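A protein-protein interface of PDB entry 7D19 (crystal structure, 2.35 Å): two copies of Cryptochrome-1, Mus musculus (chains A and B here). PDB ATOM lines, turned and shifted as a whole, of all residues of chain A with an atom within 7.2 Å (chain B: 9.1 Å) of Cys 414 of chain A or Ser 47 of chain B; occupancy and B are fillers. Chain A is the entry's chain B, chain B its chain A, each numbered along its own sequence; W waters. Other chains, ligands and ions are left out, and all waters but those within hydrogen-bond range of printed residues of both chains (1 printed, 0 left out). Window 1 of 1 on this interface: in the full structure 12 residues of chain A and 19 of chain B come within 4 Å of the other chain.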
ATOM      1  N   CYS A 365      -8.008   5.932 -30.318  1.00  0.00           N
ATOM      2  CA  CYS A 365      -8.954   6.397 -29.310  1.00  0.00           C
ATOM      3  C   CYS A 365      -9.225   5.313 -28.274  1.00  0.00           C
ATOM      4  O   CYS A 365      -9.259   5.593 -27.069  1.00  0.00           O
ATOM      5  CB  CYS A 365     -10.249   6.852 -29.990  1.00  0.00           C
ATOM      6  SG  CYS A 365     -11.619   7.258 -28.866  1.00  0.00           S
ATOM      7  N   PHE A 366      -9.403   4.067 -28.727  1.00  0.00           N
ATOM      8  CA  PHE A 366      -9.599   2.949 -27.809  1.00  0.00           C
ATOM      9  C   PHE A 366      -8.451   2.834 -26.815  1.00  0.00           C
ATOM     10  O   PHE A 366      -8.670   2.580 -25.625  1.00  0.00           O
ATOM     11  CB  PHE A 366      -9.741   1.648 -28.602  1.00  0.00           C
ATOM     12  CG  PHE A 366     -10.067   0.438 -27.757  1.00  0.00           C
ATOM     13  CD1 PHE A 366     -11.363   0.195 -27.346  1.00  0.00           C
ATOM     14  CD2 PHE A 366      -9.077  -0.457 -27.389  1.00  0.00           C
ATOM     15  CE1 PHE A 366     -11.670  -0.918 -26.572  1.00  0.00           C
ATOM     16  CE2 PHE A 366      -9.379  -1.572 -26.631  1.00  0.00           C
ATOM     17  CZ  PHE A 366     -10.679  -1.797 -26.214  1.00  0.00           C
ATOM     18  N   ARG A 369      -7.608   8.018 -25.056  1.00  0.00           N
ATOM     19  CA  ARG A 369      -8.646   8.796 -24.386  1.00  0.00           C
ATOM     20  C   ARG A 369      -9.969   8.049 -24.260  1.00  0.00           C
ATOM     21  O   ARG A 369     -10.789   8.414 -23.414  1.00  0.00           O
ATOM     22  CB  ARG A 369      -8.877  10.109 -25.136  1.00  0.00           C
ATOM     23  CG  ARG A 369      -9.282   9.895 -26.585  1.00  0.00           C
ATOM     24  CD  ARG A 369      -9.286  11.190 -27.364  1.00  0.00           C
ATOM     25  NE  ARG A 369      -9.803  10.995 -28.716  1.00  0.00           N
ATOM     26  CZ  ARG A 369     -11.080  11.146 -29.033  1.00  0.00           C
ATOM     27  NH1 ARG A 369     -11.944  11.497 -28.091  1.00  0.00           N
ATOM     28  NH2 ARG A 369     -11.489  10.949 -30.276  1.00  0.00           N
ATOM     29  N   GLY A 370     -10.203   7.028 -25.076  1.00  0.00           N
ATOM     30  CA  GLY A 370     -11.485   6.347 -25.068  1.00  0.00           C
ATOM     31  C   GLY A 370     -11.656   5.337 -23.952  1.00  0.00           C
ATOM     32  O   GLY A 370     -12.496   5.520 -23.064  1.00  0.00           O
ATOM     33  N   ASP A 371     -10.866   4.265 -23.971  1.00  0.00           N
ATOM     34  CA  ASP A 371     -11.119   3.138 -23.081  1.00  0.00           C
ATOM     35  C   ASP A 371      -9.979   2.874 -22.106  1.00  0.00           C
ATOM     36  O   ASP A 371     -10.217   2.825 -20.895  1.00  0.00           O
ATOM     37  CB  ASP A 371     -11.405   1.887 -23.912  1.00  0.00           C
ATOM     38  CG  ASP A 371     -12.673   2.009 -24.708  1.00  0.00           C
ATOM     39  OD1 ASP A 371     -12.731   2.889 -25.580  1.00  0.00           O
ATOM     40  OD2 ASP A 371     -13.613   1.230 -24.468  1.00  0.00           O
ATOM     41  N   PHE A 411     -11.110  17.008 -29.296  1.00  0.00           N
ATOM     42  CA  PHE A 411     -12.109  16.235 -30.009  1.00  0.00           C
ATOM     43  C   PHE A 411     -13.354  16.098 -29.143  1.00  0.00           C
ATOM     44  O   PHE A 411     -13.265  15.749 -27.962  1.00  0.00           O
ATOM     45  CB  PHE A 411     -11.547  14.869 -30.407  1.00  0.00           C
ATOM     46  CG  PHE A 411     -10.599  14.930 -31.567  1.00  0.00           C
ATOM     47  CD1 PHE A 411     -11.048  15.333 -32.816  1.00  0.00           C
ATOM     48  CD2 PHE A 411      -9.262  14.597 -31.416  1.00  0.00           C
ATOM     49  CE1 PHE A 411     -10.182  15.404 -33.894  1.00  0.00           C
ATOM     50  CE2 PHE A 411      -8.391  14.664 -32.491  1.00  0.00           C
ATOM     51  CZ  PHE A 411      -8.853  15.068 -33.734  1.00  0.00           C
ATOM     52  N   PHE A 412     -14.510  16.403 -29.726  1.00  0.00           N
ATOM     53  CA  PHE A 412     -15.779  16.236 -29.032  1.00  0.00           C
ATOM     54  C   PHE A 412     -16.350  14.837 -29.195  1.00  0.00           C
ATOM     55  O   PHE A 412     -17.313  14.495 -28.504  1.00  0.00           O
ATOM     56  CB  PHE A 412     -16.795  17.262 -29.535  1.00  0.00           C
ATOM     57  CG  PHE A 412     -16.572  18.644 -29.009  1.00  0.00           C
ATOM     58  CD1 PHE A 412     -15.487  19.390 -29.428  1.00  0.00           C
ATOM     59  CD2 PHE A 412     -17.463  19.206 -28.108  1.00  0.00           C
ATOM     60  CE1 PHE A 412     -15.280  20.668 -28.950  1.00  0.00           C
ATOM     61  CE2 PHE A 412     -17.264  20.484 -27.619  1.00  0.00           C
ATOM     62  CZ  PHE A 412     -16.167  21.218 -28.042  1.00  0.00           C
ATOM     63  N   HIS A 413     -15.765  14.026 -30.073  1.00  0.00           N
ATOM     64  CA  HIS A 413     -16.279  12.711 -30.437  1.00  0.00           C
ATOM     65  C   HIS A 413     -15.401  11.602 -29.869  1.00  0.00           C
ATOM     66  O   HIS A 413     -14.173  11.721 -29.858  1.00  0.00           O
ATOM     67  CB  HIS A 413     -16.361  12.571 -31.960  1.00  0.00           C
ATOM     68  CG  HIS A 413     -16.603  11.168 -32.427  1.00  0.00           C
ATOM     69  ND1 HIS A 413     -15.671  10.452 -33.149  1.00  0.00           N
ATOM     70  CD2 HIS A 413     -17.669  10.349 -32.271  1.00  0.00           C
ATOM     71  CE1 HIS A 413     -16.157   9.254 -33.423  1.00  0.00           C
ATOM     72  NE2 HIS A 413     -17.366   9.165 -32.897  1.00  0.00           N
ATOM     73  N   CYS A 414     -16.033  10.518 -29.414  1.00  0.00           N
ATOM     74  CA  CYS A 414     -15.332   9.353 -28.883  1.00  0.00           C
ATOM     75  C   CYS A 414     -15.861   8.108 -29.581  1.00  0.00           C
ATOM     76  O   CYS A 414     -17.057   7.814 -29.501  1.00  0.00           O
ATOM     77  CB  CYS A 414     -15.534   9.239 -27.367  1.00  0.00           C
ATOM     78  SG  CYS A 414     -14.859   7.733 -26.593  1.00  0.00           S
ATOM     79  N   TYR A 415     -14.972   7.358 -30.229  1.00  0.00           N
ATOM     80  CA  TYR A 415     -15.385   6.225 -31.052  1.00  0.00           C
ATOM     81  C   TYR A 415     -16.039   5.129 -30.211  1.00  0.00           C
ATOM     82  O   TYR A 415     -15.740   4.965 -29.027  1.00  0.00           O
ATOM     83  CB  TYR A 415     -14.176   5.658 -31.817  1.00  0.00           C
ATOM     84  CG  TYR A 415     -13.743   6.578 -32.931  1.00  0.00           C
ATOM     85  CD1 TYR A 415     -14.380   6.552 -34.162  1.00  0.00           C
ATOM     86  CD2 TYR A 415     -12.725   7.507 -32.736  1.00  0.00           C
ATOM     87  CE1 TYR A 415     -14.001   7.409 -35.175  1.00  0.00           C
ATOM     88  CE2 TYR A 415     -12.346   8.363 -33.741  1.00  0.00           C
ATOM     89  CZ  TYR A 415     -12.985   8.311 -34.960  1.00  0.00           C
ATOM     90  OH  TYR A 415     -12.613   9.171 -35.967  1.00  0.00           O
ATOM     91  N   CYS A 416     -16.953   4.380 -30.836  1.00  0.00           N
ATOM     92  CA  CYS A 416     -17.558   3.214 -30.203  1.00  0.00           C
ATOM     93  C   CYS A 416     -16.901   1.945 -30.733  1.00  0.00           C
ATOM     94  O   CYS A 416     -16.966   1.683 -31.945  1.00  0.00           O
ATOM     95  CB  CYS A 416     -19.066   3.171 -30.452  1.00  0.00           C
ATOM     96  SG  CYS A 416     -19.866   1.682 -29.784  1.00  0.00           S
ATOM     97  N   PRO A 417     -16.272   1.135 -29.869  1.00  0.00           N
ATOM     98  CA  PRO A 417     -15.591  -0.084 -30.351  1.00  0.00           C
ATOM     99  C   PRO A 417     -16.525  -1.112 -30.965  1.00  0.00           C
ATOM    100  O   PRO A 417     -16.078  -1.927 -31.779  1.00  0.00           O
ATOM    101  CB  PRO A 417     -14.917  -0.639 -29.087  1.00  0.00           C
ATOM    102  CG  PRO A 417     -15.669  -0.020 -27.940  1.00  0.00           C
ATOM    103  CD  PRO A 417     -16.070   1.348 -28.427  1.00  0.00           C
ATOM    104  N   GLY A 419     -19.873  -0.020 -32.146  1.00  0.00           N
ATOM    105  CA  GLY A 419     -20.765   0.655 -33.076  1.00  0.00           C
ATOM    106  C   GLY A 419     -20.073   1.084 -34.353  1.00  0.00           C
ATOM    107  O   GLY A 419     -20.624   0.935 -35.447  1.00  0.00           O
ATOM    108  N   HIS A 475     -17.223  -0.621 -22.116  1.00  0.00           N
ATOM    109  CA  HIS A 475     -16.964   0.646 -22.793  1.00  0.00           C
ATOM    110  C   HIS A 475     -17.769   1.780 -22.177  1.00  0.00           C
ATOM    111  O   HIS A 475     -17.243   2.882 -21.973  1.00  0.00           O
ATOM    112  CB  HIS A 475     -17.273   0.536 -24.284  1.00  0.00           C
ATOM    113  CG  HIS A 475     -17.037   1.809 -25.033  1.00  0.00           C
ATOM    114  ND1 HIS A 475     -15.780   2.351 -25.204  1.00  0.00           N
ATOM    115  CD2 HIS A 475     -17.900   2.663 -25.631  1.00  0.00           C
ATOM    116  CE1 HIS A 475     -15.878   3.476 -25.890  1.00  0.00           C
ATOM    117  NE2 HIS A 475     -17.154   3.689 -26.160  1.00  0.00           N
ATOM    118  N   SER A 479     -15.428   4.528 -20.918  1.00  0.00           N
ATOM    119  CA  SER A 479     -15.383   5.754 -21.706  1.00  0.00           C
ATOM    120  C   SER A 479     -15.950   6.938 -20.932  1.00  0.00           C
ATOM    121  O   SER A 479     -15.398   8.042 -20.991  1.00  0.00           O
ATOM    122  CB  SER A 479     -16.115   5.566 -23.033  1.00  0.00           C
ATOM    123  OG  SER A 479     -17.503   5.431 -22.833  1.00  0.00           O
ATOM    124  N   ARG A 480     -17.046   6.733 -20.192  1.00  0.00           N
ATOM    125  CA  ARG A 480     -17.618   7.842 -19.430  1.00  0.00           C
ATOM    126  C   ARG A 480     -16.601   8.410 -18.442  1.00  0.00           C
ATOM    127  O   ARG A 480     -16.450   9.634 -18.325  1.00  0.00           O
ATOM    128  CB  ARG A 480     -18.886   7.389 -18.702  1.00  0.00           C
ATOM    129  N   ASN A 482     -13.278   8.148 -18.640  1.00  0.00           N
ATOM    130  CA  ASN A 482     -12.207   8.781 -19.385  1.00  0.00           C
ATOM    131  C   ASN A 482     -12.661  10.101 -19.991  1.00  0.00           C
ATOM    132  O   ASN A 482     -11.875  11.054 -20.058  1.00  0.00           O
ATOM    133  CB  ASN A 482     -11.692   7.815 -20.443  1.00  0.00           C
ATOM    134  CG  ASN A 482     -11.037   6.588 -19.823  1.00  0.00           C
ATOM    135  OD1 ASN A 482     -10.558   6.639 -18.684  1.00  0.00           O
ATOM    136  ND2 ASN A 482     -10.999   5.487 -20.570  1.00  0.00           N
ATOM    137  N   ILE A 483     -13.923  10.191 -20.409  1.00  0.00           N
ATOM    138  CA  ILE A 483     -14.447  11.470 -20.880  1.00  0.00           C
ATOM    139  C   ILE A 483     -14.432  12.493 -19.746  1.00  0.00           C
ATOM    140  O   ILE A 483     -14.034  13.649 -19.939  1.00  0.00           O
ATOM    141  CB  ILE A 483     -15.855  11.278 -21.484  1.00  0.00           C
ATOM    142  CG1 ILE A 483     -15.755  10.548 -22.832  1.00  0.00           C
ATOM    143  CG2 ILE A 483     -16.584  12.612 -21.640  1.00  0.00           C
ATOM    144  CD1 ILE A 483     -17.008   9.779 -23.205  1.00  0.00           C
ATOM    145  N   PHE B  43     -19.705  19.774 -23.509  1.00  0.00           N
ATOM    146  CA  PHE B  43     -20.604  18.956 -24.307  1.00  0.00           C
ATOM    147  C   PHE B  43     -19.883  17.840 -25.066  1.00  0.00           C
ATOM    148  O   PHE B  43     -20.518  17.141 -25.863  1.00  0.00           O
ATOM    149  CB  PHE B  43     -21.384  19.845 -25.280  1.00  0.00           C
ATOM    150  N   ALA B  44     -18.588  17.646 -24.822  1.00  0.00           N
ATOM    151  CA  ALA B  44     -17.803  16.643 -25.524  1.00  0.00           C
ATOM    152  C   ALA B  44     -18.132  15.234 -25.022  1.00  0.00           C
ATOM    153  O   ALA B  44     -18.810  15.042 -24.006  1.00  0.00           O
ATOM    154  CB  ALA B  44     -16.312  16.925 -25.360  1.00  0.00           C
ATOM    155  N   GLY B  45     -17.630  14.239 -25.754  1.00  0.00           N
ATOM    156  CA  GLY B  45     -17.799  12.848 -25.389  1.00  0.00           C
ATOM    157  C   GLY B  45     -18.844  12.088 -26.178  1.00  0.00           C
ATOM    158  O   GLY B  45     -19.016  10.886 -25.942  1.00  0.00           O
ATOM    159  N   SER B  46     -19.545  12.745 -27.099  1.00  0.00           N
ATOM    160  CA  SER B  46     -20.542  12.067 -27.916  1.00  0.00           C
ATOM    161  C   SER B  46     -19.871  11.079 -28.868  1.00  0.00           C
ATOM    162  O   SER B  46     -18.751  11.292 -29.338  1.00  0.00           O
ATOM    163  CB  SER B  46     -21.356  13.089 -28.716  1.00  0.00           C
ATOM    164  OG  SER B  46     -22.476  13.560 -27.983  1.00  0.00           O
ATOM    165  N   SER B  47     -20.561   9.979 -29.150  1.00  0.00           N
ATOM    166  CA  SER B  47     -20.098   9.086 -30.197  1.00  0.00           C
ATOM    167  C   SER B  47     -20.698   9.546 -31.526  1.00  0.00           C
ATOM    168  O   SER B  47     -21.421  10.543 -31.594  1.00  0.00           O
ATOM    169  CB  SER B  47     -20.447   7.631 -29.869  1.00  0.00           C
ATOM    170  OG  SER B  47     -21.613   7.192 -30.549  1.00  0.00           O
ATOM    171  N   ASN B  48     -20.396   8.815 -32.603  1.00  0.00           N
ATOM    172  CA  ASN B  48     -20.915   9.180 -33.920  1.00  0.00           C
ATOM    173  C   ASN B  48     -22.443   9.200 -33.971  1.00  0.00           C
ATOM    174  O   ASN B  48     -23.005   9.749 -34.925  1.00  0.00           O
ATOM    175  CB  ASN B  48     -20.361   8.228 -34.988  1.00  0.00           C
ATOM    176  CG  ASN B  48     -19.156   8.811 -35.721  1.00  0.00           C
ATOM    177  OD1 ASN B  48     -19.198   9.944 -36.196  1.00  0.00           O
ATOM    178  ND2 ASN B  48     -18.075   8.039 -35.805  1.00  0.00           N
ATOM    179  N   VAL B  49     -23.121   8.637 -32.968  1.00  0.00           N
ATOM    180  CA  VAL B  49     -24.579   8.643 -32.952  1.00  0.00           C
ATOM    181  C   VAL B  49     -25.115  10.062 -32.825  1.00  0.00           C
ATOM    182  O   VAL B  49     -26.203  10.365 -33.332  1.00  0.00           O
ATOM    183  CB  VAL B  49     -25.102   7.739 -31.820  1.00  0.00           C
ATOM    184  N   GLY B  50     -24.370  10.954 -32.168  1.00  0.00           N
ATOM    185  CA  GLY B  50     -24.819  12.316 -31.923  1.00  0.00           C
ATOM    186  C   GLY B  50     -24.491  13.292 -33.036  1.00  0.00           C
ATOM    187  O   GLY B  50     -24.497  14.514 -32.832  1.00  0.00           O
ATOM    188  N   ILE B  51     -24.256  12.766 -34.238  1.00  0.00           N
ATOM    189  CA  ILE B  51     -23.718  13.589 -35.317  1.00  0.00           C
ATOM    190  C   ILE B  51     -24.760  14.556 -35.880  1.00  0.00           C
ATOM    191  O   ILE B  51     -24.410  15.654 -36.341  1.00  0.00           O
ATOM    192  CB  ILE B  51     -23.136  12.686 -36.413  1.00  0.00           C
ATOM    193  CG1 ILE B  51     -22.358  13.515 -37.442  1.00  0.00           C
ATOM    194  CG2 ILE B  51     -24.239  11.842 -37.057  1.00  0.00           C
ATOM    195  CD1 ILE B  51     -21.536  12.653 -38.385  1.00  0.00           C
ATOM    196  N   ASN B  52     -26.046  14.194 -35.835  1.00  0.00           N
ATOM    197  CA  ASN B  52     -27.049  15.028 -36.490  1.00  0.00           C
ATOM    198  C   ASN B  52     -27.254  16.337 -35.733  1.00  0.00           C
ATOM    199  O   ASN B  52     -27.424  17.394 -36.351  1.00  0.00           O
ATOM    200  CB  ASN B  52     -28.354  14.245 -36.653  1.00  0.00           C
ATOM    201  CG  ASN B  52     -28.257  13.172 -37.747  1.00  0.00           C
ATOM    202  OD1 ASN B  52     -27.497  13.317 -38.709  1.00  0.00           O
ATOM    203  ND2 ASN B  52     -29.020  12.097 -37.599  1.00  0.00           N
ATOM    204  N   ARG B  53     -27.194  16.293 -34.399  1.00  0.00           N
ATOM    205  CA  ARG B  53     -27.269  17.505 -33.595  1.00  0.00           C
ATOM    206  C   ARG B  53     -26.076  18.405 -33.874  1.00  0.00           C
ATOM    207  O   ARG B  53     -26.228  19.610 -34.066  1.00  0.00           O
ATOM    208  CB  ARG B  53     -27.327  17.151 -32.103  1.00  0.00           C
ATOM    209  CG  ARG B  53     -28.570  17.654 -31.395  1.00  0.00           C
ATOM    210  CD  ARG B  53     -28.535  17.383 -29.889  1.00  0.00           C
ATOM    211  NE  ARG B  53     -27.867  18.453 -29.149  1.00  0.00           N
ATOM    212  CZ  ARG B  53     -27.927  18.613 -27.829  1.00  0.00           C
ATOM    213  NH1 ARG B  53     -27.275  19.622 -27.263  1.00  0.00           N
ATOM    214  NH2 ARG B  53     -28.631  17.771 -27.076  1.00  0.00           N
ATOM    215  N   TRP B  54     -24.877  17.835 -33.877  1.00  0.00           N
ATOM    216  CA  TRP B  54     -23.691  18.631 -34.154  1.00  0.00           C
ATOM    217  C   TRP B  54     -23.733  19.202 -35.561  1.00  0.00           C
ATOM    218  O   TRP B  54     -23.439  20.387 -35.755  1.00  0.00           O
ATOM    219  CB  TRP B  54     -22.436  17.789 -33.945  1.00  0.00           C
ATOM    220  CG  TRP B  54     -22.080  17.652 -32.505  1.00  0.00           C
ATOM    221  CD1 TRP B  54     -22.161  16.516 -31.727  1.00  0.00           C
ATOM    222  CD2 TRP B  54     -21.586  18.685 -31.652  1.00  0.00           C
ATOM    223  NE1 TRP B  54     -21.729  16.792 -30.450  1.00  0.00           N
ATOM    224  CE2 TRP B  54     -21.360  18.108 -30.379  1.00  0.00           C
ATOM    225  CE3 TRP B  54     -21.268  20.027 -31.851  1.00  0.00           C
ATOM    226  CZ2 TRP B  54     -20.852  18.838 -29.308  1.00  0.00           C
ATOM    227  CZ3 TRP B  54     -20.772  20.757 -30.779  1.00  0.00           C
ATOM    228  CH2 TRP B  54     -20.575  20.164 -29.525  1.00  0.00           C
ATOM    229  N   LEU B 200     -14.350  18.211 -35.000  1.00  0.00           N
ATOM    230  CA  LEU B 200     -14.856  17.749 -33.715  1.00  0.00           C
ATOM    231  C   LEU B 200     -14.682  16.249 -33.524  1.00  0.00           C
ATOM    232  O   LEU B 200     -15.079  15.721 -32.477  1.00  0.00           O
ATOM    233  CB  LEU B 200     -16.331  18.118 -33.560  1.00  0.00           C
ATOM    234  CG  LEU B 200     -16.653  19.567 -33.911  1.00  0.00           C
ATOM    235  CD1 LEU B 200     -18.150  19.810 -33.828  1.00  0.00           C
ATOM    236  CD2 LEU B 200     -15.894  20.533 -33.014  1.00  0.00           C
ATOM    237  N   GLY B 201     -14.113  15.553 -34.505  1.00  0.00           N
ATOM    238  CA  GLY B 201     -13.868  14.140 -34.380  1.00  0.00           C
ATOM    239  C   GLY B 201     -14.910  13.221 -34.976  1.00  0.00           C
ATOM    240  O   GLY B 201     -14.802  12.004 -34.792  1.00  0.00           O
ATOM    241  N   PHE B 202     -15.894  13.741 -35.701  1.00  0.00           N
ATOM    242  CA  PHE B 202     -16.944  12.898 -36.251  1.00  0.00           C
ATOM    243  C   PHE B 202     -16.554  12.341 -37.612  1.00  0.00           C
ATOM    244  O   PHE B 202     -15.881  13.008 -38.403  1.00  0.00           O
ATOM    245  CB  PHE B 202     -18.256  13.670 -36.349  1.00  0.00           C
ATOM    246  CG  PHE B 202     -18.855  13.950 -35.017  1.00  0.00           C
ATOM    247  CD1 PHE B 202     -19.457  12.928 -34.293  1.00  0.00           C
ATOM    248  CD2 PHE B 202     -18.753  15.204 -34.447  1.00  0.00           C
ATOM    249  CE1 PHE B 202     -19.985  13.173 -33.042  1.00  0.00           C
ATOM    250  CE2 PHE B 202     -19.273  15.449 -33.203  1.00  0.00           C
ATOM    251  CZ  PHE B 202     -19.882  14.432 -32.498  1.00  0.00           C
ATOM    252  N   ASP B 203     -16.979  11.101 -37.865  1.00  0.00           N
ATOM    253  CA  ASP B 203     -16.771  10.439 -39.149  1.00  0.00           C
ATOM    254  C   ASP B 203     -17.841  10.899 -40.130  1.00  0.00           C
ATOM    255  O   ASP B 203     -19.037  10.711 -39.888  1.00  0.00           O
ATOM    256  CB  ASP B 203     -16.815   8.921 -38.977  1.00  0.00           C
ATOM    257  N   GLU B 334     -31.027   1.040 -30.215  1.00  0.00           N
ATOM    258  CA  GLU B 334     -30.456   0.707 -31.515  1.00  0.00           C
ATOM    259  C   GLU B 334     -31.489   0.187 -32.505  1.00  0.00           C
ATOM    260  O   GLU B 334     -31.111  -0.223 -33.608  1.00  0.00           O
ATOM    261  CB  GLU B 334     -29.340  -0.329 -31.349  1.00  0.00           C
ATOM    262  CG  GLU B 334     -28.102   0.235 -30.674  1.00  0.00           C
ATOM    263  CD  GLU B 334     -27.251  -0.826 -30.003  1.00  0.00           C
ATOM    264  OE1 GLU B 334     -27.514  -2.030 -30.208  1.00  0.00           O
ATOM    265  OE2 GLU B 334     -26.312  -0.447 -29.270  1.00  0.00           O
ATOM    266  N   ARG B 350     -32.401   7.764 -35.401  1.00  0.00           N
ATOM    267  CA  ARG B 350     -30.943   7.729 -35.463  1.00  0.00           C
ATOM    268  C   ARG B 350     -30.427   8.359 -36.747  1.00  0.00           C
ATOM    269  O   ARG B 350     -29.435   9.094 -36.731  1.00  0.00           O
ATOM    270  CB  ARG B 350     -30.435   6.288 -35.354  1.00  0.00           C
ATOM    271  CG  ARG B 350     -30.225   5.770 -33.944  1.00  0.00           C
ATOM    272  CD  ARG B 350     -29.090   4.725 -33.869  1.00  0.00           C
ATOM    273  NE  ARG B 350     -28.953   4.182 -32.517  1.00  0.00           N
ATOM    274  CZ  ARG B 350     -28.369   4.824 -31.510  1.00  0.00           C
ATOM    275  NH1 ARG B 350     -27.856   6.030 -31.701  1.00  0.00           N
ATOM    276  NH2 ARG B 350     -28.292   4.262 -30.313  1.00  0.00           N
ATOM    277  N   GLU B 385     -29.461  12.863 -27.097  1.00  0.00           N
ATOM    278  CA  GLU B 385     -28.387  12.737 -28.063  1.00  0.00           C
ATOM    279  C   GLU B 385     -28.883  12.690 -29.509  1.00  0.00           C
ATOM    280  O   GLU B 385     -28.175  13.138 -30.417  1.00  0.00           O
ATOM    281  CB  GLU B 385     -27.529  11.504 -27.765  1.00  0.00           C
ATOM    282  CG  GLU B 385     -26.120  11.631 -28.325  1.00  0.00           C
ATOM    283  CD  GLU B 385     -25.325  12.771 -27.681  1.00  0.00           C
ATOM    284  OE1 GLU B 385     -24.892  13.707 -28.404  1.00  0.00           O
ATOM    285  OE2 GLU B 385     -25.113  12.719 -26.456  1.00  0.00           O
ATOM    286  N   LEU B 386     -30.090  12.200 -29.765  1.00  0.00           N
ATOM    287  CA  LEU B 386     -30.511  11.945 -31.140  1.00  0.00           C
ATOM    288  C   LEU B 386     -31.508  12.955 -31.697  1.00  0.00           C
ATOM    289  O   LEU B 386     -31.516  13.178 -32.908  1.00  0.00           O
ATOM    290  CB  LEU B 386     -31.125  10.542 -31.262  1.00  0.00           C
ATOM    291  CG  LEU B 386     -30.263   9.298 -30.968  1.00  0.00           C
ATOM    292  CD1 LEU B 386     -31.089   8.005 -31.197  1.00  0.00           C
ATOM    293  CD2 LEU B 386     -28.980   9.247 -31.786  1.00  0.00           C
HETATM  294  O   HOH W   1     -18.381   6.033 -33.202  1.00  0.00           O
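Cys 414 of chain A touches just these residues of chain B: Ser 46 (2.8 Å) and Ser 47 (3.4 Å).
Gly 370 of chain A touches none of the printed residues of chain B.
His 413 of chain A touches just these residues of chain B: Ser 46 (3.1 Å), Ser 47 (3.2 Å), Asn 48 (3.1 Å), Leu 200 (3.0 Å), Gly 201 (2.4 Å) and Phe 202 (3.7 Å).
Of the printed residues of chain A, Trp 54 of chain B touches Phe 412 (3.6 Å).
Of the printed residues of chain B, Phe 412 of chain A touches Ala 44 (3.7 Å), Gly 45 (2.8 Å), Ser 46 (3.2 Å), Trp 54 (3.6 Å) and Leu 200 (2.9 Å).
Of the printed residues of chain A, Phe 202 of chain B touches His 413.
Printed residues of chain A within 4 Å of Asn 48 of chain B: His 413 (3.1 Å).
Printed residues of chain A within 4 Å of Ser 46 of chain B: Phe 412 (3.2 Å), His 413 (3.1 Å) and Cys 414 (2.8 Å).
The nearest residue of chain B that does not touch Cys 414 of chain A is Gly 45 of chain B (4.1 Å).
The nearest residue of chain A that does not touch Ser 47 of chain B is Cys 416 of chain A (4.7 Å).
The backbone carbonyl oxygen (O) of Tyr 415 of chain A is in hydrogen-bond range of a ring nitrogen (NE2) of His 475 of chain A (3.4 Å).
OG of Ser 46 of chain B is in hydrogen-bond range of OE1 of Glu 385 of chain B.
The side-chain sulfur of Cys 365 of chain A lies within hydrogen-bond range of the backbone NH of Tyr 415 of chain A, at 3.6 Å.
The backbone carbonyl oxygen (O) of His 413 of chain A is in hydrogen-bond range of the guanidinium group (NH2) of Arg 369 of chain A, 2.8 Å away.
The side-chain amide oxygen of Asn 48 of chain B sits at hydrogen-bond distance from the backbone NH of Asp 203 of chain B, 3.0 Å away.
The backbone NH (N) of Val 49 of chain B lies close to the side-chain hydroxyl (OG) of Ser 47 of chain B (3.2 Å).
The backbone carbonyl oxygen (O) of Gly 201 of chain B is in hydrogen-bond range of a ring nitrogen (ND1) of His 413 of chain A, 2.4 Å away.
O of Phe 412 of chain A is in hydrogen-bond range of N of Gly 45 of chain B.
O of Phe 412 of chain A lies within hydrogen-bond range of N of Ser 46 of chain B (3.2 Å).
O of Leu 200 of chain B sits at hydrogen-bond distance from N of His 413 of chain A (3.0 Å).
The backbone carbonyl oxygen (O) of Ser 46 of chain B sits at hydrogen-bond distance from the backbone NH (N) of Cys 414 of chain A (2.8 Å).
O of Leu 200 of chain B sits at hydrogen-bond distance from N of Phe 412 of chain A (2.9 Å).
A ring nitrogen (NE2) of His 413 of chain A sits at hydrogen-bond distance from the backbone NH (N) of Asn 48 of chain B (3.1 Å).
Of the 18 printed residues of chain A, 6 touch a printed residue of chain B.
Hydrophobic or aromatic side chains of chain A that line the printed part of chain B: Phe 411, Phe 412, His 413, Tyr 415 and Ile 483.
Of the 20 printed residues of chain B, 9 touch a printed residue of chain A.
Hydrophobic or aromatic side chains of chain B within 4 Å of the printed part of chain A: Ala 44, Trp 54, Leu 200 and Phe 202.
Among the printed residues, 17 pairs touch across the chains.
Among the printed residues, merely in contact across the chains: His 413 of chain A with Ser 46 of chain B (3.1 Å), His 413 of chain A with Ser 47 of chain B (3.2 Å), Cys 414 of chain A with Ser 47 of chain B (3.4 Å), Phe 411 of chain A with Gly 201 of chain B (3.4 Å), Phe 412 of chain A with Trp 54 of chain B (3.6 Å), Ile 483 of chain A with Gly 45 of chain B (3.6 Å), Phe 412 of chain A with Ala 44 of chain B (3.7 Å), His 413 of chain A with Phe 202 of chain B (3.7 Å), Tyr 415 of chain A with Gly 201 of chain B (3.8 Å) and Phe 411 of chain A with Leu 200 of chain B (3.8 Å).
No position is printed for both chains.
Of the 17 pairs that touch across the chains among the printed residues, none has its exchanged pair printed and touching as well.
Water W1 lies within hydrogen-bond range of the backbone NH (N) of Cys 416 of chain A (3.2 Å), the side-chain amide nitrogen (ND2) of Asn 48 of chain B (3.3 Å) and a ring nitrogen (NE2) of His 413 of chain A (3.3 Å).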
